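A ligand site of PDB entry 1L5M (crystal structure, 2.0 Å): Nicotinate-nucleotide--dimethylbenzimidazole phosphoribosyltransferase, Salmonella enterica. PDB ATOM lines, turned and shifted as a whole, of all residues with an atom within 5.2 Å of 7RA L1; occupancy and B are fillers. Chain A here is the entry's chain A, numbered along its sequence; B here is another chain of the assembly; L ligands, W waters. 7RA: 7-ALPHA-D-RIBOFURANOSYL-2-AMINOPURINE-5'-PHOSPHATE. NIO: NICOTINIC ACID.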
ATOM      1  N   VAL A  77       0.278 -30.024  -2.979  1.00  0.00           N
ATOM      2  CA  VAL A  77       0.039 -28.605  -3.257  1.00  0.00           C
ATOM      3  C   VAL A  77       0.492 -27.636  -2.153  1.00  0.00           C
ATOM      4  O   VAL A  77       0.393 -26.414  -2.321  1.00  0.00           O
ATOM      5  CB  VAL A  77      -1.472 -28.343  -3.514  1.00  0.00           C
ATOM      6  CG1 VAL A  77      -1.928 -29.139  -4.725  1.00  0.00           C
ATOM      7  CG2 VAL A  77      -2.297 -28.738  -2.281  1.00  0.00           C
ATOM      8  N   ALA A  78       0.970 -28.182  -1.027  1.00  0.00           N
ATOM      9  CA  ALA A  78       1.424 -27.370   0.113  1.00  0.00           C
ATOM     10  C   ALA A  78       2.773 -27.876   0.628  1.00  0.00           C
ATOM     11  O   ALA A  78       2.971 -29.074   0.773  1.00  0.00           O
ATOM     12  CB  ALA A  78       0.390 -27.412   1.244  1.00  0.00           C
ATOM     13  N   SER A  80       4.109 -27.235   3.706  1.00  0.00           N
ATOM     14  CA  SER A  80       4.158 -27.544   5.128  1.00  0.00           C
ATOM     15  C   SER A  80       3.476 -28.879   5.457  1.00  0.00           C
ATOM     16  O   SER A  80       2.488 -29.241   4.836  1.00  0.00           O
ATOM     17  CB  SER A  80       3.459 -26.440   5.940  1.00  0.00           C
ATOM     18  OG  SER A  80       3.788 -25.136   5.483  1.00  0.00           O
ATOM     19  N   VAL A  84       0.992 -29.031  10.719  1.00  0.00           N
ATOM     20  CA  VAL A  84       1.144 -27.621  11.026  1.00  0.00           C
ATOM     21  C   VAL A  84      -0.216 -26.976  11.319  1.00  0.00           C
ATOM     22  O   VAL A  84      -0.280 -26.018  12.079  1.00  0.00           O
ATOM     23  CB  VAL A  84       1.890 -26.885   9.884  1.00  0.00           C
ATOM     24  CG1 VAL A  84       1.878 -25.368  10.124  1.00  0.00           C
ATOM     25  CG2 VAL A  84       3.312 -27.394   9.812  1.00  0.00           C
ATOM     26  N   GLN A  88      -0.511 -24.855  14.785  1.00  0.00           N
ATOM     27  CA  GLN A  88      -0.840 -23.449  14.791  1.00  0.00           C
ATOM     28  C   GLN A  88      -2.165 -23.178  15.514  1.00  0.00           C
ATOM     29  O   GLN A  88      -2.340 -22.122  16.109  1.00  0.00           O
ATOM     30  CB  GLN A  88      -0.877 -22.913  13.361  1.00  0.00           C
ATOM     31  CG  GLN A  88       0.502 -22.663  12.783  1.00  0.00           C
ATOM     32  CD  GLN A  88       1.216 -21.512  13.459  1.00  0.00           C
ATOM     33  OE1 GLN A  88       1.615 -21.593  14.630  1.00  0.00           O
ATOM     34  NE2 GLN A  88       1.383 -20.413  12.736  1.00  0.00           N
ATOM     35  N   GLU A 174      -8.803 -17.938   8.916  1.00  0.00           N
ATOM     36  CA  GLU A 174      -8.709 -19.376   8.760  1.00  0.00           C
ATOM     37  C   GLU A 174      -7.314 -19.935   9.039  1.00  0.00           C
ATOM     38  O   GLU A 174      -6.354 -19.187   9.240  1.00  0.00           O
ATOM     39  CB  GLU A 174      -9.125 -19.778   7.336  1.00  0.00           C
ATOM     40  CG  GLU A 174      -8.554 -18.868   6.242  1.00  0.00           C
ATOM     41  CD  GLU A 174      -7.032 -18.800   6.286  1.00  0.00           C
ATOM     42  OE1 GLU A 174      -6.392 -19.867   6.141  1.00  0.00           O
ATOM     43  OE2 GLU A 174      -6.481 -17.699   6.478  1.00  0.00           O
ATOM     44  N   LEU A 175      -7.241 -21.262   9.069  1.00  0.00           N
ATOM     45  CA  LEU A 175      -6.003 -21.990   9.271  1.00  0.00           C
ATOM     46  C   LEU A 175      -6.238 -23.378   8.665  1.00  0.00           C
ATOM     47  O   LEU A 175      -7.192 -24.074   9.035  1.00  0.00           O
ATOM     48  CB  LEU A 175      -5.715 -22.121  10.767  1.00  0.00           C
ATOM     49  CG  LEU A 175      -4.275 -22.397  11.199  1.00  0.00           C
ATOM     50  CD1 LEU A 175      -3.347 -21.300  10.600  1.00  0.00           C
ATOM     51  CD2 LEU A 175      -4.195 -22.408  12.743  1.00  0.00           C
ATOM     52  N   GLY A 176      -5.398 -23.768   7.716  1.00  0.00           N
ATOM     53  CA  GLY A 176      -5.543 -25.081   7.094  1.00  0.00           C
ATOM     54  C   GLY A 176      -4.546 -25.255   5.958  1.00  0.00           C
ATOM     55  O   GLY A 176      -4.686 -24.623   4.907  1.00  0.00           O
ATOM     56  N   MET A 177      -3.534 -26.097   6.187  1.00  0.00           N
ATOM     57  CA  MET A 177      -2.517 -26.319   5.176  1.00  0.00           C
ATOM     58  C   MET A 177      -3.193 -26.764   3.882  1.00  0.00           C
ATOM     59  O   MET A 177      -4.113 -27.601   3.889  1.00  0.00           O
ATOM     60  CB  MET A 177      -1.509 -27.392   5.624  1.00  0.00           C
ATOM     61  CG  MET A 177      -0.744 -27.043   6.909  1.00  0.00           C
ATOM     62  SD  MET A 177       0.001 -25.385   6.885  1.00  0.00           S
ATOM     63  CE  MET A 177      -1.079 -24.526   8.026  1.00  0.00           C
ATOM     64  N   ALA A 178      -2.738 -26.174   2.782  1.00  0.00           N
ATOM     65  CA  ALA A 178      -3.258 -26.458   1.454  1.00  0.00           C
ATOM     66  C   ALA A 178      -4.567 -25.744   1.106  1.00  0.00           C
ATOM     67  O   ALA A 178      -5.080 -25.945   0.006  1.00  0.00           O
ATOM     68  CB  ALA A 178      -3.455 -27.972   1.277  1.00  0.00           C
ATOM     69  N   ASN A 179      -5.108 -24.908   1.991  1.00  0.00           N
ATOM     70  CA  ASN A 179      -6.376 -24.275   1.649  1.00  0.00           C
ATOM     71  C   ASN A 179      -6.388 -23.228   0.532  1.00  0.00           C
ATOM     72  O   ASN A 179      -7.473 -22.844   0.094  1.00  0.00           O
ATOM     73  CB  ASN A 179      -7.149 -23.776   2.900  1.00  0.00           C
ATOM     74  CG  ASN A 179      -6.534 -22.563   3.596  1.00  0.00           C
ATOM     75  OD1 ASN A 179      -5.572 -21.957   3.120  1.00  0.00           O
ATOM     76  ND2 ASN A 179      -7.110 -22.202   4.749  1.00  0.00           N
ATOM     77  N   THR A 180      -5.226 -22.784   0.038  1.00  0.00           N
ATOM     78  CA  THR A 180      -5.268 -21.832  -1.068  1.00  0.00           C
ATOM     79  C   THR A 180      -5.587 -22.574  -2.370  1.00  0.00           C
ATOM     80  O   THR A 180      -5.886 -21.955  -3.384  1.00  0.00           O
ATOM     81  CB  THR A 180      -3.956 -21.013  -1.243  1.00  0.00           C
ATOM     82  OG1 THR A 180      -2.862 -21.893  -1.538  1.00  0.00           O
ATOM     83  CG2 THR A 180      -3.654 -20.216   0.026  1.00  0.00           C
ATOM     84  N   THR A 181      -5.556 -23.905  -2.345  1.00  0.00           N
ATOM     85  CA  THR A 181      -5.906 -24.672  -3.538  1.00  0.00           C
ATOM     86  C   THR A 181      -7.436 -24.628  -3.758  1.00  0.00           C
ATOM     87  O   THR A 181      -7.883 -24.204  -4.816  1.00  0.00           O
ATOM     88  CB  THR A 181      -5.380 -26.107  -3.467  1.00  0.00           C
ATOM     89  OG1 THR A 181      -3.949 -26.060  -3.550  1.00  0.00           O
ATOM     90  CG2 THR A 181      -5.925 -26.963  -4.613  1.00  0.00           C
ATOM     91  N   ILE A 201       1.217 -18.869  -5.055  1.00  0.00           N
ATOM     92  CA  ILE A 201       2.220 -19.612  -4.289  1.00  0.00           C
ATOM     93  C   ILE A 201       1.802 -19.961  -2.844  1.00  0.00           C
ATOM     94  O   ILE A 201       2.571 -20.589  -2.112  1.00  0.00           O
ATOM     95  CB  ILE A 201       3.543 -18.829  -4.280  1.00  0.00           C
ATOM     96  N   GLY A 202       0.596 -19.552  -2.438  1.00  0.00           N
ATOM     97  CA  GLY A 202       0.144 -19.878  -1.087  1.00  0.00           C
ATOM     98  C   GLY A 202       1.223 -19.549  -0.056  1.00  0.00           C
ATOM     99  O   GLY A 202       1.807 -18.464  -0.091  1.00  0.00           O
ATOM    100  N   ALA A 203       1.497 -20.485   0.848  1.00  0.00           N
ATOM    101  CA  ALA A 203       2.504 -20.279   1.877  1.00  0.00           C
ATOM    102  C   ALA A 203       3.869 -20.724   1.356  1.00  0.00           C
ATOM    103  O   ALA A 203       4.349 -21.818   1.661  1.00  0.00           O
ATOM    104  CB  ALA A 203       2.120 -21.065   3.152  1.00  0.00           C
ATOM    105  N   LYS A 213       0.000 -27.590  -8.944  1.00  0.00           N
ATOM    106  CA  LYS A 213      -1.133 -26.964  -8.271  1.00  0.00           C
ATOM    107  C   LYS A 213      -2.188 -26.525  -9.280  1.00  0.00           C
ATOM    108  O   LYS A 213      -3.377 -26.730  -9.060  1.00  0.00           O
ATOM    109  CB  LYS A 213      -0.647 -25.778  -7.424  1.00  0.00           C
ATOM    110  CG  LYS A 213      -1.681 -25.212  -6.458  1.00  0.00           C
ATOM    111  CD  LYS A 213      -1.028 -24.243  -5.479  1.00  0.00           C
ATOM    112  CE  LYS A 213      -2.066 -23.427  -4.714  1.00  0.00           C
ATOM    113  NZ  LYS A 213      -1.387 -22.423  -3.824  1.00  0.00           N
ATOM    114  N   LEU A 266      -8.203 -16.304   0.997  1.00  0.00           N
ATOM    115  CA  LEU A 266      -9.157 -17.326   1.420  1.00  0.00           C
ATOM    116  C   LEU A 266     -10.527 -16.708   1.703  1.00  0.00           C
ATOM    117  O   LEU A 266     -11.566 -17.272   1.348  1.00  0.00           O
ATOM    118  CB  LEU A 266      -8.680 -18.044   2.694  1.00  0.00           C
ATOM    119  CG  LEU A 266      -7.437 -18.946   2.683  1.00  0.00           C
ATOM    120  CD1 LEU A 266      -7.408 -19.794   1.394  1.00  0.00           C
ATOM    121  CD2 LEU A 266      -6.180 -18.117   2.784  1.00  0.00           C
ATOM    122  N   LEU A 315      -0.479 -13.894   4.988  1.00  0.00           N
ATOM    123  CA  LEU A 315      -0.384 -14.816   6.098  1.00  0.00           C
ATOM    124  C   LEU A 315      -1.706 -15.536   6.358  1.00  0.00           C
ATOM    125  O   LEU A 315      -1.710 -16.711   6.676  1.00  0.00           O
ATOM    126  CB  LEU A 315       0.060 -14.084   7.361  1.00  0.00           C
ATOM    127  CG  LEU A 315      -0.040 -14.870   8.689  1.00  0.00           C
ATOM    128  CD1 LEU A 315       0.873 -16.087   8.644  1.00  0.00           C
ATOM    129  CD2 LEU A 315       0.353 -13.951   9.850  1.00  0.00           C
ATOM    130  N   GLY A 316      -2.818 -14.820   6.236  1.00  0.00           N
ATOM    131  CA  GLY A 316      -4.100 -15.450   6.526  1.00  0.00           C
ATOM    132  C   GLY A 316      -4.352 -15.308   8.026  1.00  0.00           C
ATOM    133  O   GLY A 316      -3.856 -14.368   8.653  1.00  0.00           O
ATOM    134  N   GLU A 317      -5.101 -16.246   8.594  1.00  0.00           N
ATOM    135  CA  GLU A 317      -5.444 -16.249  10.022  1.00  0.00           C
ATOM    136  C   GLU A 317      -6.394 -15.147  10.451  1.00  0.00           C
ATOM    137  O   GLU A 317      -6.845 -15.123  11.607  1.00  0.00           O
ATOM    138  CB  GLU A 317      -4.182 -16.122  10.885  1.00  0.00           C
ATOM    139  CG  GLU A 317      -3.036 -17.034  10.465  1.00  0.00           C
ATOM    140  CD  GLU A 317      -1.884 -16.981  11.452  1.00  0.00           C
ATOM    141  OE1 GLU A 317      -1.955 -16.152  12.387  1.00  0.00           O
ATOM    142  OE2 GLU A 317      -0.915 -17.749  11.283  1.00  0.00           O
ATOM    143  N   LEU B  30       6.797 -17.282  14.106  1.00  0.00           N
ATOM    144  CA  LEU B  30       5.818 -18.341  13.846  1.00  0.00           C
ATOM    145  C   LEU B  30       4.926 -18.071  12.616  1.00  0.00           C
ATOM    146  O   LEU B  30       3.705 -17.912  12.729  1.00  0.00           O
ATOM    147  CB  LEU B  30       4.960 -18.503  15.086  1.00  0.00           C
ATOM    148  CG  LEU B  30       4.339 -19.844  15.480  1.00  0.00           C
ATOM    149  CD1 LEU B  30       5.405 -20.921  15.562  1.00  0.00           C
ATOM    150  CD2 LEU B  30       3.635 -19.665  16.830  1.00  0.00           C
ATOM    151  N   LYS B  31       5.547 -18.033  11.451  1.00  0.00           N
ATOM    152  CA  LYS B  31       4.810 -17.749  10.223  1.00  0.00           C
ATOM    153  C   LYS B  31       5.714 -18.067   9.046  1.00  0.00           C
ATOM    154  O   LYS B  31       6.929 -18.146   9.201  1.00  0.00           O
ATOM    155  CB  LYS B  31       4.469 -16.267  10.156  1.00  0.00           C
ATOM    156  CG  LYS B  31       5.729 -15.408  10.216  1.00  0.00           C
ATOM    157  CD  LYS B  31       5.447 -13.922  10.043  1.00  0.00           C
ATOM    158  CE  LYS B  31       6.723 -13.125  10.197  1.00  0.00           C
ATOM    159  NZ  LYS B  31       7.742 -13.559   9.205  1.00  0.00           N
ATOM    160  N   PRO B  32       5.125 -18.249   7.859  1.00  0.00           N
ATOM    161  CA  PRO B  32       5.933 -18.538   6.673  1.00  0.00           C
ATOM    162  C   PRO B  32       6.792 -17.292   6.433  1.00  0.00           C
ATOM    163  O   PRO B  32       6.298 -16.175   6.518  1.00  0.00           O
ATOM    164  CB  PRO B  32       4.896 -18.707   5.569  1.00  0.00           C
ATOM    165  CG  PRO B  32       3.696 -19.242   6.324  1.00  0.00           C
ATOM    166  CD  PRO B  32       3.693 -18.397   7.575  1.00  0.00           C
ATOM    167  N   LEU B 341       9.331 -19.979  15.550  1.00  0.00           N
ATOM    168  CA  LEU B 341       9.204 -21.277  14.899  1.00  0.00           C
ATOM    169  C   LEU B 341       9.978 -22.350  15.639  1.00  0.00           C
ATOM    170  O   LEU B 341       9.510 -23.481  15.796  1.00  0.00           O
ATOM    171  CB  LEU B 341       9.707 -21.184  13.460  1.00  0.00           C
ATOM    172  CG  LEU B 341       8.798 -20.477  12.453  1.00  0.00           C
ATOM    173  CD1 LEU B 341       9.585 -20.118  11.198  1.00  0.00           C
ATOM    174  CD2 LEU B 341       7.603 -21.374  12.128  1.00  0.00           C
ATOM    175  N   ILE B 346       8.531 -26.560  14.281  1.00  0.00           N
ATOM    176  CA  ILE B 346       8.082 -26.362  12.900  1.00  0.00           C
ATOM    177  C   ILE B 346       9.283 -26.007  12.022  1.00  0.00           C
ATOM    178  O   ILE B 346      10.082 -25.145  12.385  1.00  0.00           O
ATOM    179  CB  ILE B 346       7.024 -25.219  12.806  1.00  0.00           C
ATOM    180  CG1 ILE B 346       5.840 -25.511  13.733  1.00  0.00           C
ATOM    181  CG2 ILE B 346       6.513 -25.101  11.373  1.00  0.00           C
ATOM    182  CD1 ILE B 346       4.831 -24.382  13.795  1.00  0.00           C
HETATM  183  C4  7RA L   1       0.287 -20.108   8.977  1.00  0.00           C
HETATM  184  C5  7RA L   1       0.044 -20.473   7.636  1.00  0.00           C
HETATM  185  C6  7RA L   1       0.926 -21.411   7.013  1.00  0.00           C
HETATM  186  N1  7RA L   1       1.964 -21.905   7.783  1.00  0.00           N
HETATM  187  C2  7RA L   1       2.155 -21.509   9.088  1.00  0.00           C
HETATM  188  N3  7RA L   1       1.324 -20.617   9.696  1.00  0.00           N
HETATM  189  N9  7RA L   1      -0.660 -19.225   9.304  1.00  0.00           N
HETATM  190  C8  7RA L   1      -1.426 -19.036   8.239  1.00  0.00           C
HETATM  191  N7  7RA L   1      -1.055 -19.786   7.175  1.00  0.00           N
HETATM  192  N10 7RA L   1       3.220 -22.039   9.821  1.00  0.00           N
HETATM  193  P   7RA L   1      -1.021 -23.176   1.449  1.00  0.00           P
HETATM  194  O1P 7RA L   1      -2.213 -23.428   0.566  1.00  0.00           O
HETATM  195  O2P 7RA L   1       0.225 -23.021   0.673  1.00  0.00           O
HETATM  196  O3P 7RA L   1      -0.868 -24.313   2.391  1.00  0.00           O
HETATM  197  O5' 7RA L   1      -1.296 -21.801   2.244  1.00  0.00           O
HETATM  198  C5' 7RA L   1      -2.483 -21.633   3.063  1.00  0.00           C
HETATM  199  C4' 7RA L   1      -2.102 -21.775   4.516  1.00  0.00           C
HETATM  200  O4' 7RA L   1      -1.114 -20.775   4.960  1.00  0.00           O
HETATM  201  C3' 7RA L   1      -3.231 -21.626   5.531  1.00  0.00           C
HETATM  202  O3' 7RA L   1      -2.985 -22.345   6.755  1.00  0.00           O
HETATM  203  C2' 7RA L   1      -3.199 -20.137   5.745  1.00  0.00           C
HETATM  204  O2' 7RA L   1      -3.915 -19.750   6.925  1.00  0.00           O
HETATM  205  C1' 7RA L   1      -1.711 -19.804   5.775  1.00  0.00           C
HETATM  206  N   NIO L   2      -2.135 -17.797   3.149  1.00  0.00           N
HETATM  207  C1  NIO L   2      -3.088 -16.803   3.271  1.00  0.00           C
HETATM  208  C2  NIO L   2      -3.158 -15.845   2.242  1.00  0.00           C
HETATM  209  C3  NIO L   2      -2.272 -15.914   1.063  1.00  0.00           C
HETATM  210  C4  NIO L   2      -1.353 -16.986   1.073  1.00  0.00           C
HETATM  211  C5  NIO L   2      -1.228 -17.969   2.076  1.00  0.00           C
HETATM  212  C6  NIO L   2      -4.209 -14.728   2.341  1.00  0.00           C
HETATM  213  O1  NIO L   2      -4.291 -13.874   1.416  1.00  0.00           O
HETATM  214  O2  NIO L   2      -5.000 -14.657   3.367  1.00  0.00           O
HETATM  215  O   HOH W   1       1.675 -24.989   3.232  1.00  0.00           O
HETATM  216  O   HOH W   2       0.600 -23.604  -2.125  1.00  0.00           O
HETATM  217  O   HOH W   3      -2.164 -25.230  -1.487  1.00  0.00           O
HETATM  218  O   HOH W   4       2.776 -24.052   0.826  1.00  0.00           O
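The backbone NH (N) of Ala 203 lies within hydrogen-bond range of an oxygen (O2P) of 7RA L1, 2.8 Å away.
The backbone NH of Thr 180 sits at hydrogen-bond distance from an oxygen (O1P) of 7RA L1.
N3 of 7RA L1 lies within hydrogen-bond range of NE2 of Gln 88 (3.0 Å).
The side-chain carboxylate (OE1) of Glu 174 is in hydrogen-bond range of an oxygen (O2') of 7RA L1, 2.6 Å away.
The backbone carbonyl oxygen of Gly 176 lies close to an oxygen (O3') of 7RA L1, 3.4 Å away.
O3P of 7RA L1 is in hydrogen-bond range of N of Ala 178 (2.7 Å).
The side-chain hydroxyl (OG1) of Thr 180 is in hydrogen-bond range of an oxygen (O1P) of 7RA L1 (2.7 Å).
The side-chain carboxylate (OE2) of Glu 317 lies within hydrogen-bond range of a nitrogen (N9) of 7RA L1 (2.5 Å).
An oxygen (O3') of 7RA L1 is in hydrogen-bond range of the backbone NH (N) of Gly 176 (3.0 Å).
The backbone carbonyl oxygen (O) of Glu 174 sits close to an oxygen (O2') of 7RA L1.
The backbone NH (N) of Glu 317 lies within hydrogen-bond range of the side-chain carboxylate (OE2) of Glu 174 (2.9 Å).
NE2 of Gln 88 is in hydrogen-bond range of O of Leu 30 of chain B, 3.4 Å away.
The backbone carbonyl oxygen (O) of Gly 176 sits close to the side-chain amide oxygen (OD1) of Asn 179, at 3.3 Å.
The side-chain hydroxyl of Thr 180 sits at hydrogen-bond distance from the side-chain amino group of Lys 213, at 2.8 Å.
The side-chain carboxylate (OE1) of Glu 174 lies within hydrogen-bond range of the side-chain amide nitrogen (ND2) of Asn 179.
The backbone carbonyl oxygen of Leu 315 sits close to a nitrogen (N7) of 7RA L1 (3.2 Å).
Residues that only touch 7RA L1: Ala 78, Val 84, Leu 175, Met 177, Asn 179, Gly 202 and Pro 32 of chain B.
Hydrophobic or aromatic side chains within 4 Å of 7RA L1: Ala 78, Val 84, Leu 175, Met 177, Ala 203, Leu 315 and Pro 32 of chain B.
Of the 26 residues printed, 15 come within 4 Å of 7RA L1.
The nearest printed residue that does not touch 7RA L1 is Gly 316 (4.3 Å).
Water W3 lies within hydrogen-bond range of O1P of 7RA L1 (2.7 Å), OG1 of Thr 181 (2.9 Å), O of Val 77 (2.9 Å), O of Ala 178 (3.4 Å) and OG1 of Thr 180 (3.4 Å).
Water W4 bridges an oxygen (O2P) of 7RA L1 (2.8 Å) and the backbone carbonyl oxygen (O) of Ala 203 (2.9 Å).
Water W1 lies within hydrogen-bond range of O3P of 7RA L1 (2.8 Å) and OG of Ser 80 (3.1 Å).
Water W2 lies within hydrogen-bond range of the backbone carbonyl oxygen of Val 77 (2.8 Å), the side-chain amino group of Lys 213 (2.9 Å) and an oxygen (O2P) of 7RA L1 (2.9 Å).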
